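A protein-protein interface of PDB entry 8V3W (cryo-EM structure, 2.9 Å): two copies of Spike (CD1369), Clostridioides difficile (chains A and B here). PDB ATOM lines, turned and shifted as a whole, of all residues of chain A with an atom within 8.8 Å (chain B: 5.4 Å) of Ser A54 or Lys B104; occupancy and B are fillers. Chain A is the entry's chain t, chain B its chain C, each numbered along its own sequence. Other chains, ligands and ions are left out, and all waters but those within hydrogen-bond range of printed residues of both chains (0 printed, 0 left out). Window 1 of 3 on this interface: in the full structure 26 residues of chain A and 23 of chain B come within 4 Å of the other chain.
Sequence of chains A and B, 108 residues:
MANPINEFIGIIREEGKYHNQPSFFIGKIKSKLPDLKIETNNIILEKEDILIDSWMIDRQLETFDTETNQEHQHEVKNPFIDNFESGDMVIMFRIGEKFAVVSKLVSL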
ATOM      1  N   LEU A  51      -1.341  -2.033   2.996  1.00  0.00           N
ATOM      2  CA  LEU A  51      -1.636  -3.108   3.934  1.00  0.00           C
ATOM      3  C   LEU A  51      -2.353  -2.499   5.130  1.00  0.00           C
ATOM      4  O   LEU A  51      -1.912  -1.478   5.662  1.00  0.00           O
ATOM      5  CB  LEU A  51      -0.359  -3.816   4.389  1.00  0.00           C
ATOM      6  CG  LEU A  51       0.426  -4.618   3.354  1.00  0.00           C
ATOM      7  CD1 LEU A  51       1.711  -5.139   3.960  1.00  0.00           C
ATOM      8  CD2 LEU A  51      -0.402  -5.759   2.811  1.00  0.00           C
ATOM      9  N   ILE A  52      -3.456  -3.110   5.550  1.00  0.00           N
ATOM     10  CA  ILE A  52      -4.304  -2.497   6.563  1.00  0.00           C
ATOM     11  C   ILE A  52      -4.451  -3.431   7.757  1.00  0.00           C
ATOM     12  O   ILE A  52      -4.243  -4.641   7.667  1.00  0.00           O
ATOM     13  CB  ILE A  52      -5.686  -2.110   6.003  1.00  0.00           C
ATOM     14  CG1 ILE A  52      -6.239  -0.897   6.753  1.00  0.00           C
ATOM     15  CG2 ILE A  52      -6.644  -3.285   6.072  1.00  0.00           C
ATOM     16  CD1 ILE A  52      -7.462  -0.294   6.120  1.00  0.00           C
ATOM     17  N   ASP A  53      -4.799  -2.833   8.891  1.00  0.00           N
ATOM     18  CA  ASP A  53      -5.091  -3.586  10.101  1.00  0.00           C
ATOM     19  C   ASP A  53      -6.330  -4.451   9.900  1.00  0.00           C
ATOM     20  O   ASP A  53      -7.290  -4.047   9.242  1.00  0.00           O
ATOM     21  CB  ASP A  53      -5.300  -2.620  11.268  1.00  0.00           C
ATOM     22  CG  ASP A  53      -5.353  -3.315  12.613  1.00  0.00           C
ATOM     23  OD1 ASP A  53      -5.801  -4.475  12.688  1.00  0.00           O
ATOM     24  OD2 ASP A  53      -4.955  -2.684  13.612  1.00  0.00           O
ATOM     25  N   SER A  54      -6.309  -5.647  10.489  1.00  0.00           N
ATOM     26  CA  SER A  54      -7.420  -6.579  10.324  1.00  0.00           C
ATOM     27  C   SER A  54      -8.696  -6.057  10.975  1.00  0.00           C
ATOM     28  O   SER A  54      -9.792  -6.234  10.430  1.00  0.00           O
ATOM     29  CB  SER A  54      -7.042  -7.939  10.901  1.00  0.00           C
ATOM     30  OG  SER A  54      -6.338  -7.785  12.116  1.00  0.00           O
ATOM     31  N   TRP A  55      -8.577  -5.417  12.141  1.00  0.00           N
ATOM     32  CA  TRP A  55      -9.763  -4.933  12.842  1.00  0.00           C
ATOM     33  C   TRP A  55     -10.518  -3.894  12.030  1.00  0.00           C
ATOM     34  O   TRP A  55     -11.744  -3.800  12.134  1.00  0.00           O
ATOM     35  CB  TRP A  55      -9.377  -4.353  14.201  1.00  0.00           C
ATOM     36  CG  TRP A  55     -10.529  -3.729  14.929  1.00  0.00           C
ATOM     37  CD1 TRP A  55     -10.625  -2.437  15.354  1.00  0.00           C
ATOM     38  CD2 TRP A  55     -11.756  -4.365  15.307  1.00  0.00           C
ATOM     39  NE1 TRP A  55     -11.829  -2.232  15.981  1.00  0.00           N
ATOM     40  CE2 TRP A  55     -12.541  -3.401  15.965  1.00  0.00           C
ATOM     41  CE3 TRP A  55     -12.263  -5.658  15.160  1.00  0.00           C
ATOM     42  CZ2 TRP A  55     -13.804  -3.688  16.466  1.00  0.00           C
ATOM     43  CZ3 TRP A  55     -13.517  -5.939  15.662  1.00  0.00           C
ATOM     44  CH2 TRP A  55     -14.272  -4.961  16.308  1.00  0.00           C
ATOM     45  N   MET A  56      -9.810  -3.108  11.222  1.00  0.00           N
ATOM     46  CA  MET A  56     -10.479  -2.120  10.384  1.00  0.00           C
ATOM     47  C   MET A  56     -11.412  -2.790   9.388  1.00  0.00           C
ATOM     48  O   MET A  56     -12.517  -2.298   9.132  1.00  0.00           O
ATOM     49  CB  MET A  56      -9.441  -1.262   9.665  1.00  0.00           C
ATOM     50  CG  MET A  56      -9.091   0.020  10.390  1.00  0.00           C
ATOM     51  SD  MET A  56      -7.529   0.713   9.822  1.00  0.00           S
ATOM     52  CE  MET A  56      -7.218   1.936  11.083  1.00  0.00           C
ATOM     53  N   ILE A  57     -10.983  -3.907   8.804  1.00  0.00           N
ATOM     54  CA  ILE A  57     -11.838  -4.639   7.877  1.00  0.00           C
ATOM     55  C   ILE A  57     -12.943  -5.369   8.628  1.00  0.00           C
ATOM     56  O   ILE A  57     -14.088  -5.435   8.166  1.00  0.00           O
ATOM     57  CB  ILE A  57     -10.989  -5.604   7.031  1.00  0.00           C
ATOM     58  CG1 ILE A  57     -10.069  -4.814   6.104  1.00  0.00           C
ATOM     59  CG2 ILE A  57     -11.874  -6.530   6.220  1.00  0.00           C
ATOM     60  CD1 ILE A  57     -10.693  -3.555   5.558  1.00  0.00           C
ATOM     61  N   ASP A  58     -12.622  -5.923   9.798  1.00  0.00           N
ATOM     62  CA  ASP A  58     -13.581  -6.755  10.518  1.00  0.00           C
ATOM     63  C   ASP A  58     -14.780  -5.951  11.005  1.00  0.00           C
ATOM     64  O   ASP A  58     -15.917  -6.432  10.946  1.00  0.00           O
ATOM     65  CB  ASP A  58     -12.890  -7.443  11.693  1.00  0.00           C
ATOM     66  CG  ASP A  58     -11.930  -8.526  11.249  1.00  0.00           C
ATOM     67  OD1 ASP A  58     -11.856  -8.791  10.033  1.00  0.00           O
ATOM     68  OD2 ASP A  58     -11.247  -9.111  12.112  1.00  0.00           O
ATOM     69  N   ARG A  59     -14.552  -4.730  11.489  1.00  0.00           N
ATOM     70  CA  ARG A  59     -15.613  -3.962  12.131  1.00  0.00           C
ATOM     71  C   ARG A  59     -16.666  -3.453  11.156  1.00  0.00           C
ATOM     72  O   ARG A  59     -17.709  -2.970  11.605  1.00  0.00           O
ATOM     73  CB  ARG A  59     -15.019  -2.780  12.896  1.00  0.00           C
ATOM     74  CG  ARG A  59     -14.558  -1.640  12.011  1.00  0.00           C
ATOM     75  CD  ARG A  59     -13.806  -0.592  12.808  1.00  0.00           C
ATOM     76  NE  ARG A  59     -14.635   0.006  13.845  1.00  0.00           N
ATOM     77  CZ  ARG A  59     -14.419   1.200  14.377  1.00  0.00           C
ATOM     78  NH1 ARG A  59     -13.405   1.955  13.990  1.00  0.00           N
ATOM     79  NH2 ARG A  59     -15.241   1.650  15.319  1.00  0.00           N
ATOM     80  N   GLN A  60     -16.432  -3.535   9.851  1.00  0.00           N
ATOM     81  CA  GLN A  60     -17.444  -3.112   8.885  1.00  0.00           C
ATOM     82  C   GLN A  60     -18.391  -4.254   8.539  1.00  0.00           C
ATOM     83  O   GLN A  60     -18.665  -4.535   7.375  1.00  0.00           O
ATOM     84  CB  GLN A  60     -16.781  -2.558   7.630  1.00  0.00           C
ATOM     85  CG  GLN A  60     -15.409  -1.962   7.861  1.00  0.00           C
ATOM     86  CD  GLN A  60     -15.467  -0.602   8.516  1.00  0.00           C
ATOM     87  OE1 GLN A  60     -16.525   0.022   8.588  1.00  0.00           O
ATOM     88  NE2 GLN A  60     -14.326  -0.129   8.995  1.00  0.00           N
ATOM     89  N   ALA A 100       1.851   0.299   5.482  1.00  0.00           N
ATOM     90  CA  ALA A 100       0.980  -0.442   6.384  1.00  0.00           C
ATOM     91  C   ALA A 100       0.247   0.544   7.283  1.00  0.00           C
ATOM     92  O   ALA A 100       0.882   1.295   8.027  1.00  0.00           O
ATOM     93  CB  ALA A 100       1.779  -1.438   7.219  1.00  0.00           C
ATOM     94  N   VAL A 101      -1.080   0.520   7.231  1.00  0.00           N
ATOM     95  CA  VAL A 101      -1.911   1.453   7.984  1.00  0.00           C
ATOM     96  C   VAL A 101      -2.255   0.819   9.324  1.00  0.00           C
ATOM     97  O   VAL A 101      -2.889  -0.240   9.375  1.00  0.00           O
ATOM     98  CB  VAL A 101      -3.182   1.815   7.204  1.00  0.00           C
ATOM     99  CG1 VAL A 101      -4.079   2.702   8.042  1.00  0.00           C
ATOM    100  CG2 VAL A 101      -2.823   2.493   5.900  1.00  0.00           C
ATOM    101  N   VAL A 102      -1.858   1.473  10.408  1.00  0.00           N
ATOM    102  CA  VAL A 102      -1.965   0.905  11.746  1.00  0.00           C
ATOM    103  C   VAL A 102      -3.199   1.413  12.479  1.00  0.00           C
ATOM    104  O   VAL A 102      -3.973   0.624  13.019  1.00  0.00           O
ATOM    105  CB  VAL A 102      -0.672   1.184  12.545  1.00  0.00           C
ATOM    106  CG1 VAL A 102      -0.941   1.143  14.034  1.00  0.00           C
ATOM    107  CG2 VAL A 102       0.397   0.177  12.173  1.00  0.00           C
ATOM    108  N   MET B  56      -6.730  -7.267  21.524  1.00  0.00           N
ATOM    109  CA  MET B  56      -6.596  -8.628  21.018  1.00  0.00           C
ATOM    110  C   MET B  56      -7.084  -9.642  22.041  1.00  0.00           C
ATOM    111  O   MET B  56      -7.744 -10.622  21.688  1.00  0.00           O
ATOM    112  CB  MET B  56      -5.144  -8.905  20.646  1.00  0.00           C
ATOM    113  CG  MET B  56      -4.524  -7.827  19.791  1.00  0.00           C
ATOM    114  SD  MET B  56      -3.591  -8.483  18.406  1.00  0.00           S
ATOM    115  CE  MET B  56      -2.603  -7.065  17.973  1.00  0.00           C
ATOM    116  N   ARG B  59     -11.223  -9.124  22.665  1.00  0.00           N
ATOM    117  CA  ARG B  59     -12.188  -9.528  21.649  1.00  0.00           C
ATOM    118  C   ARG B  59     -12.430 -11.032  21.608  1.00  0.00           C
ATOM    119  O   ARG B  59     -13.376 -11.464  20.943  1.00  0.00           O
ATOM    120  CB  ARG B  59     -11.736  -9.049  20.269  1.00  0.00           C
ATOM    121  CG  ARG B  59     -10.596  -9.849  19.675  1.00  0.00           C
ATOM    122  CD  ARG B  59     -10.068  -9.208  18.407  1.00  0.00           C
ATOM    123  NE  ARG B  59     -11.088  -9.127  17.371  1.00  0.00           N
ATOM    124  CZ  ARG B  59     -10.831  -9.038  16.074  1.00  0.00           C
ATOM    125  NH1 ARG B  59      -9.591  -9.026  15.616  1.00  0.00           N
ATOM    126  NH2 ARG B  59     -11.842  -8.964  15.216  1.00  0.00           N
ATOM    127  N   ASP B  82     -11.490 -13.602  16.875  1.00  0.00           N
ATOM    128  CA  ASP B  82     -10.533 -13.930  15.822  1.00  0.00           C
ATOM    129  C   ASP B  82      -9.278 -14.451  16.505  1.00  0.00           C
ATOM    130  O   ASP B  82      -8.590 -13.697  17.198  1.00  0.00           O
ATOM    131  CB  ASP B  82     -10.236 -12.702  14.954  1.00  0.00           C
ATOM    132  CG  ASP B  82      -9.128 -12.934  13.918  1.00  0.00           C
ATOM    133  OD1 ASP B  82      -8.286 -13.842  14.067  1.00  0.00           O
ATOM    134  OD2 ASP B  82      -9.098 -12.174  12.929  1.00  0.00           O
ATOM    135  N   PHE B  84      -5.572 -15.902  15.692  1.00  0.00           N
ATOM    136  CA  PHE B  84      -4.645 -15.853  14.572  1.00  0.00           C
ATOM    137  C   PHE B  84      -4.305 -17.255  14.091  1.00  0.00           C
ATOM    138  O   PHE B  84      -4.031 -18.153  14.892  1.00  0.00           O
ATOM    139  CB  PHE B  84      -3.376 -15.111  14.968  1.00  0.00           C
ATOM    140  CG  PHE B  84      -3.633 -13.812  15.660  1.00  0.00           C
ATOM    141  CD1 PHE B  84      -4.446 -12.857  15.077  1.00  0.00           C
ATOM    142  CD2 PHE B  84      -3.061 -13.541  16.889  1.00  0.00           C
ATOM    143  CE1 PHE B  84      -4.687 -11.662  15.706  1.00  0.00           C
ATOM    144  CE2 PHE B  84      -3.298 -12.345  17.519  1.00  0.00           C
ATOM    145  CZ  PHE B  84      -4.113 -11.405  16.926  1.00  0.00           C
ATOM    146  N   ASP B  88       0.199 -15.913   9.664  1.00  0.00           N
ATOM    147  CA  ASP B  88      -0.229 -14.526   9.589  1.00  0.00           C
ATOM    148  C   ASP B  88       0.926 -13.581   9.906  1.00  0.00           C
ATOM    149  O   ASP B  88       1.933 -13.964  10.504  1.00  0.00           O
ATOM    150  CB  ASP B  88      -1.391 -14.272  10.544  1.00  0.00           C
ATOM    151  CG  ASP B  88      -2.647 -15.004  10.134  1.00  0.00           C
ATOM    152  OD1 ASP B  88      -2.628 -15.671   9.081  1.00  0.00           O
ATOM    153  OD2 ASP B  88      -3.654 -14.916  10.863  1.00  0.00           O
ATOM    154  N   MET B  89       0.755 -12.323   9.513  1.00  0.00           N
ATOM    155  CA  MET B  89       1.785 -11.303   9.623  1.00  0.00           C
ATOM    156  C   MET B  89       1.404 -10.285  10.690  1.00  0.00           C
ATOM    157  O   MET B  89       0.244  -9.877  10.781  1.00  0.00           O
ATOM    158  CB  MET B  89       1.989 -10.601   8.280  1.00  0.00           C
ATOM    159  CG  MET B  89       2.748  -9.293   8.363  1.00  0.00           C
ATOM    160  SD  MET B  89       2.583  -8.303   6.870  1.00  0.00           S
ATOM    161  CE  MET B  89       3.804  -9.081   5.826  1.00  0.00           C
ATOM    162  N   VAL B  90       2.383  -9.880  11.501  1.00  0.00           N
ATOM    163  CA  VAL B  90       2.166  -8.906  12.561  1.00  0.00           C
ATOM    164  C   VAL B  90       3.266  -7.854  12.527  1.00  0.00           C
ATOM    165  O   VAL B  90       4.358  -8.074  12.002  1.00  0.00           O
ATOM    166  CB  VAL B  90       2.108  -9.564  13.954  1.00  0.00           C
ATOM    167  CG1 VAL B  90       0.783 -10.270  14.147  1.00  0.00           C
ATOM    168  CG2 VAL B  90       3.258 -10.531  14.124  1.00  0.00           C
ATOM    169  N   ILE B  91       2.955  -6.696  13.105  1.00  0.00           N
ATOM    170  CA  ILE B  91       3.893  -5.593  13.281  1.00  0.00           C
ATOM    171  C   ILE B  91       4.215  -5.481  14.766  1.00  0.00           C
ATOM    172  O   ILE B  91       3.307  -5.448  15.605  1.00  0.00           O
ATOM    173  CB  ILE B  91       3.321  -4.279  12.712  1.00  0.00           C
ATOM    174  CG1 ILE B  91       4.359  -3.153  12.733  1.00  0.00           C
ATOM    175  CG2 ILE B  91       2.031  -3.875  13.406  1.00  0.00           C
ATOM    176  CD1 ILE B  91       5.422  -3.265  11.691  1.00  0.00           C
ATOM    177  N   VAL B 102       1.531  -4.983  18.135  1.00  0.00           N
ATOM    178  CA  VAL B 102       0.639  -3.836  18.018  1.00  0.00           C
ATOM    179  C   VAL B 102      -0.593  -4.160  17.183  1.00  0.00           C
ATOM    180  O   VAL B 102      -1.719  -3.895  17.601  1.00  0.00           O
ATOM    181  CB  VAL B 102       1.407  -2.620  17.452  1.00  0.00           C
ATOM    182  CG1 VAL B 102       0.460  -1.643  16.790  1.00  0.00           C
ATOM    183  CG2 VAL B 102       2.187  -1.940  18.557  1.00  0.00           C
ATOM    184  N   SER B 103      -0.408  -4.738  16.000  1.00  0.00           N
ATOM    185  CA  SER B 103      -1.547  -5.045  15.146  1.00  0.00           C
ATOM    186  C   SER B 103      -1.172  -6.149  14.171  1.00  0.00           C
ATOM    187  O   SER B 103       0.003  -6.455  13.970  1.00  0.00           O
ATOM    188  CB  SER B 103      -2.029  -3.804  14.392  1.00  0.00           C
ATOM    189  OG  SER B 103      -1.277  -3.604  13.211  1.00  0.00           O
ATOM    190  N   LYS B 104      -2.198  -6.741  13.567  1.00  0.00           N
ATOM    191  CA  LYS B 104      -2.044  -7.760  12.537  1.00  0.00           C
ATOM    192  C   LYS B 104      -2.431  -7.162  11.192  1.00  0.00           C
ATOM    193  O   LYS B 104      -3.447  -6.472  11.088  1.00  0.00           O
ATOM    194  CB  LYS B 104      -2.906  -8.984  12.847  1.00  0.00           C
ATOM    195  CG  LYS B 104      -3.270  -9.811  11.634  1.00  0.00           C
ATOM    196  CD  LYS B 104      -3.612 -11.226  12.036  1.00  0.00           C
ATOM    197  CE  LYS B 104      -4.608 -11.845  11.080  1.00  0.00           C
ATOM    198  NZ  LYS B 104      -5.989 -11.776  11.611  1.00  0.00           N
ATOM    199  N   LEU B 105      -1.625  -7.424  10.171  1.00  0.00           N
ATOM    200  CA  LEU B 105      -1.784  -6.797   8.868  1.00  0.00           C
ATOM    201  C   LEU B 105      -2.300  -7.808   7.857  1.00  0.00           C
ATOM    202  O   LEU B 105      -1.793  -8.930   7.781  1.00  0.00           O
ATOM    203  CB  LEU B 105      -0.459  -6.213   8.387  1.00  0.00           C
ATOM    204  CG  LEU B 105       0.323  -5.362   9.391  1.00  0.00           C
ATOM    205  CD1 LEU B 105       1.698  -5.046   8.844  1.00  0.00           C
ATOM    206  CD2 LEU B 105      -0.428  -4.088   9.725  1.00  0.00           C
ATOM    207  N   VAL B 106      -3.305  -7.406   7.081  1.00  0.00           N
ATOM    208  CA  VAL B 106      -3.803  -8.199   5.964  1.00  0.00           C
ATOM    209  C   VAL B 106      -3.874  -7.318   4.726  1.00  0.00           C
ATOM    210  O   VAL B 106      -4.028  -6.097   4.816  1.00  0.00           O
ATOM    211  CB  VAL B 106      -5.188  -8.824   6.259  1.00  0.00           C
ATOM    212  CG1 VAL B 106      -5.114  -9.720   7.487  1.00  0.00           C
ATOM    213  CG2 VAL B 106      -6.220  -7.737   6.443  1.00  0.00           C
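Ser A54 touches just one residue of chain B: Lys B104 (3.0 Å). Of chain A, only Asp A53 (3.2 Å) comes within 4 Å of Ser B103. Of the printed residues of chain B, Asp A53 touches Ser B103 (3.2 Å) and Lys B104 (3.5 Å). Printed residues of chain A within 4 Å of Asp B82: Asp A58 (3.8 Å). Printed residues of chain A within 4 Å of Leu B105: Ile A52 and Ala A100. Of the printed residues of chain B, Trp A55 touches Arg B59. Ile B91 touches none of the printed residues of chain A. The nearest residue of chain B that does not touch Ser A54 is Val B106 (4.2 Å).
Of the 13 printed residues of chain A, 7 touch a printed residue of chain B. Printed residues of chain A that touch a printed residue of chain B: Leu A51, Ile A52, Asp A53, Ser A54, Trp A55, Asp A58 and Ala A100. Hydrophobic or aromatic side chains of chain A within 4 Å of the printed part of chain B: Trp A55 and Ala A100. Of the 13 printed residues of chain B, 6 touch a printed residue of chain A. Hydrophobic or aromatic side chains of chain B within 4 Å of the printed part of chain A: Leu B105 and Val B106. Among the printed residues, Asp or Glu carboxylates within 4 Å of a Lys or Arg side-chain nitrogen of the other chain: Asp A58 with Arg B59 (3.2 Å).
Among the printed residues, pairs that only touch across the chains: Asp A53 with Ser B103 (3.2 Å), Trp A55 with Arg B59 (3.3 Å), Ile A52 with Leu B105 (3.5 Å), Asp A58 with Asp B82 (3.8 Å), Leu A51 with Val B106 (3.9 Å), Ala A100 with Leu B105 (3.96 Å) and Ile A52 with Lys B104 (3.96 Å).
NH2 of Arg B59 lies within salt-bridge range of OD2 of Asp A58 (3.2 Å). The backbone NH (N) of Ser A54 sits at hydrogen-bond distance from the backbone carbonyl oxygen (O) of Lys B104, at 3.0 Å. N of Val B106 sits at hydrogen-bond distance from O of Ile A52, 3.0 Å away. OD1 of Asp A53 lies close to O of Lys B104.
The side-chain amino group (NZ) of Lys B104 lies within salt-bridge range of the side-chain carboxylate (OD2) of Asp B82 (3.4 Å). OD2 of Asp B88 is in salt-bridge range of NZ of Lys B104. N of Ile B91 is in hydrogen-bond range of O of Ser B103 (3.1 Å). The backbone carbonyl oxygen (O) of Leu A51 is in hydrogen-bond range of the backbone NH (N) of Val A101, at 2.7 Å. The side-chain carboxylate (OD1) of Asp A53 is in hydrogen-bond range of the backbone NH (N) of Trp A55 (3.0 Å). The backbone NH of Asp A53 lies within hydrogen-bond range of the backbone carbonyl oxygen of Val A101, 3.3 Å away.
3 positions are printed for both chains. Of the 11 pairs that touch across the chains among the printed residues, none has its exchanged pair printed and touching as well.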
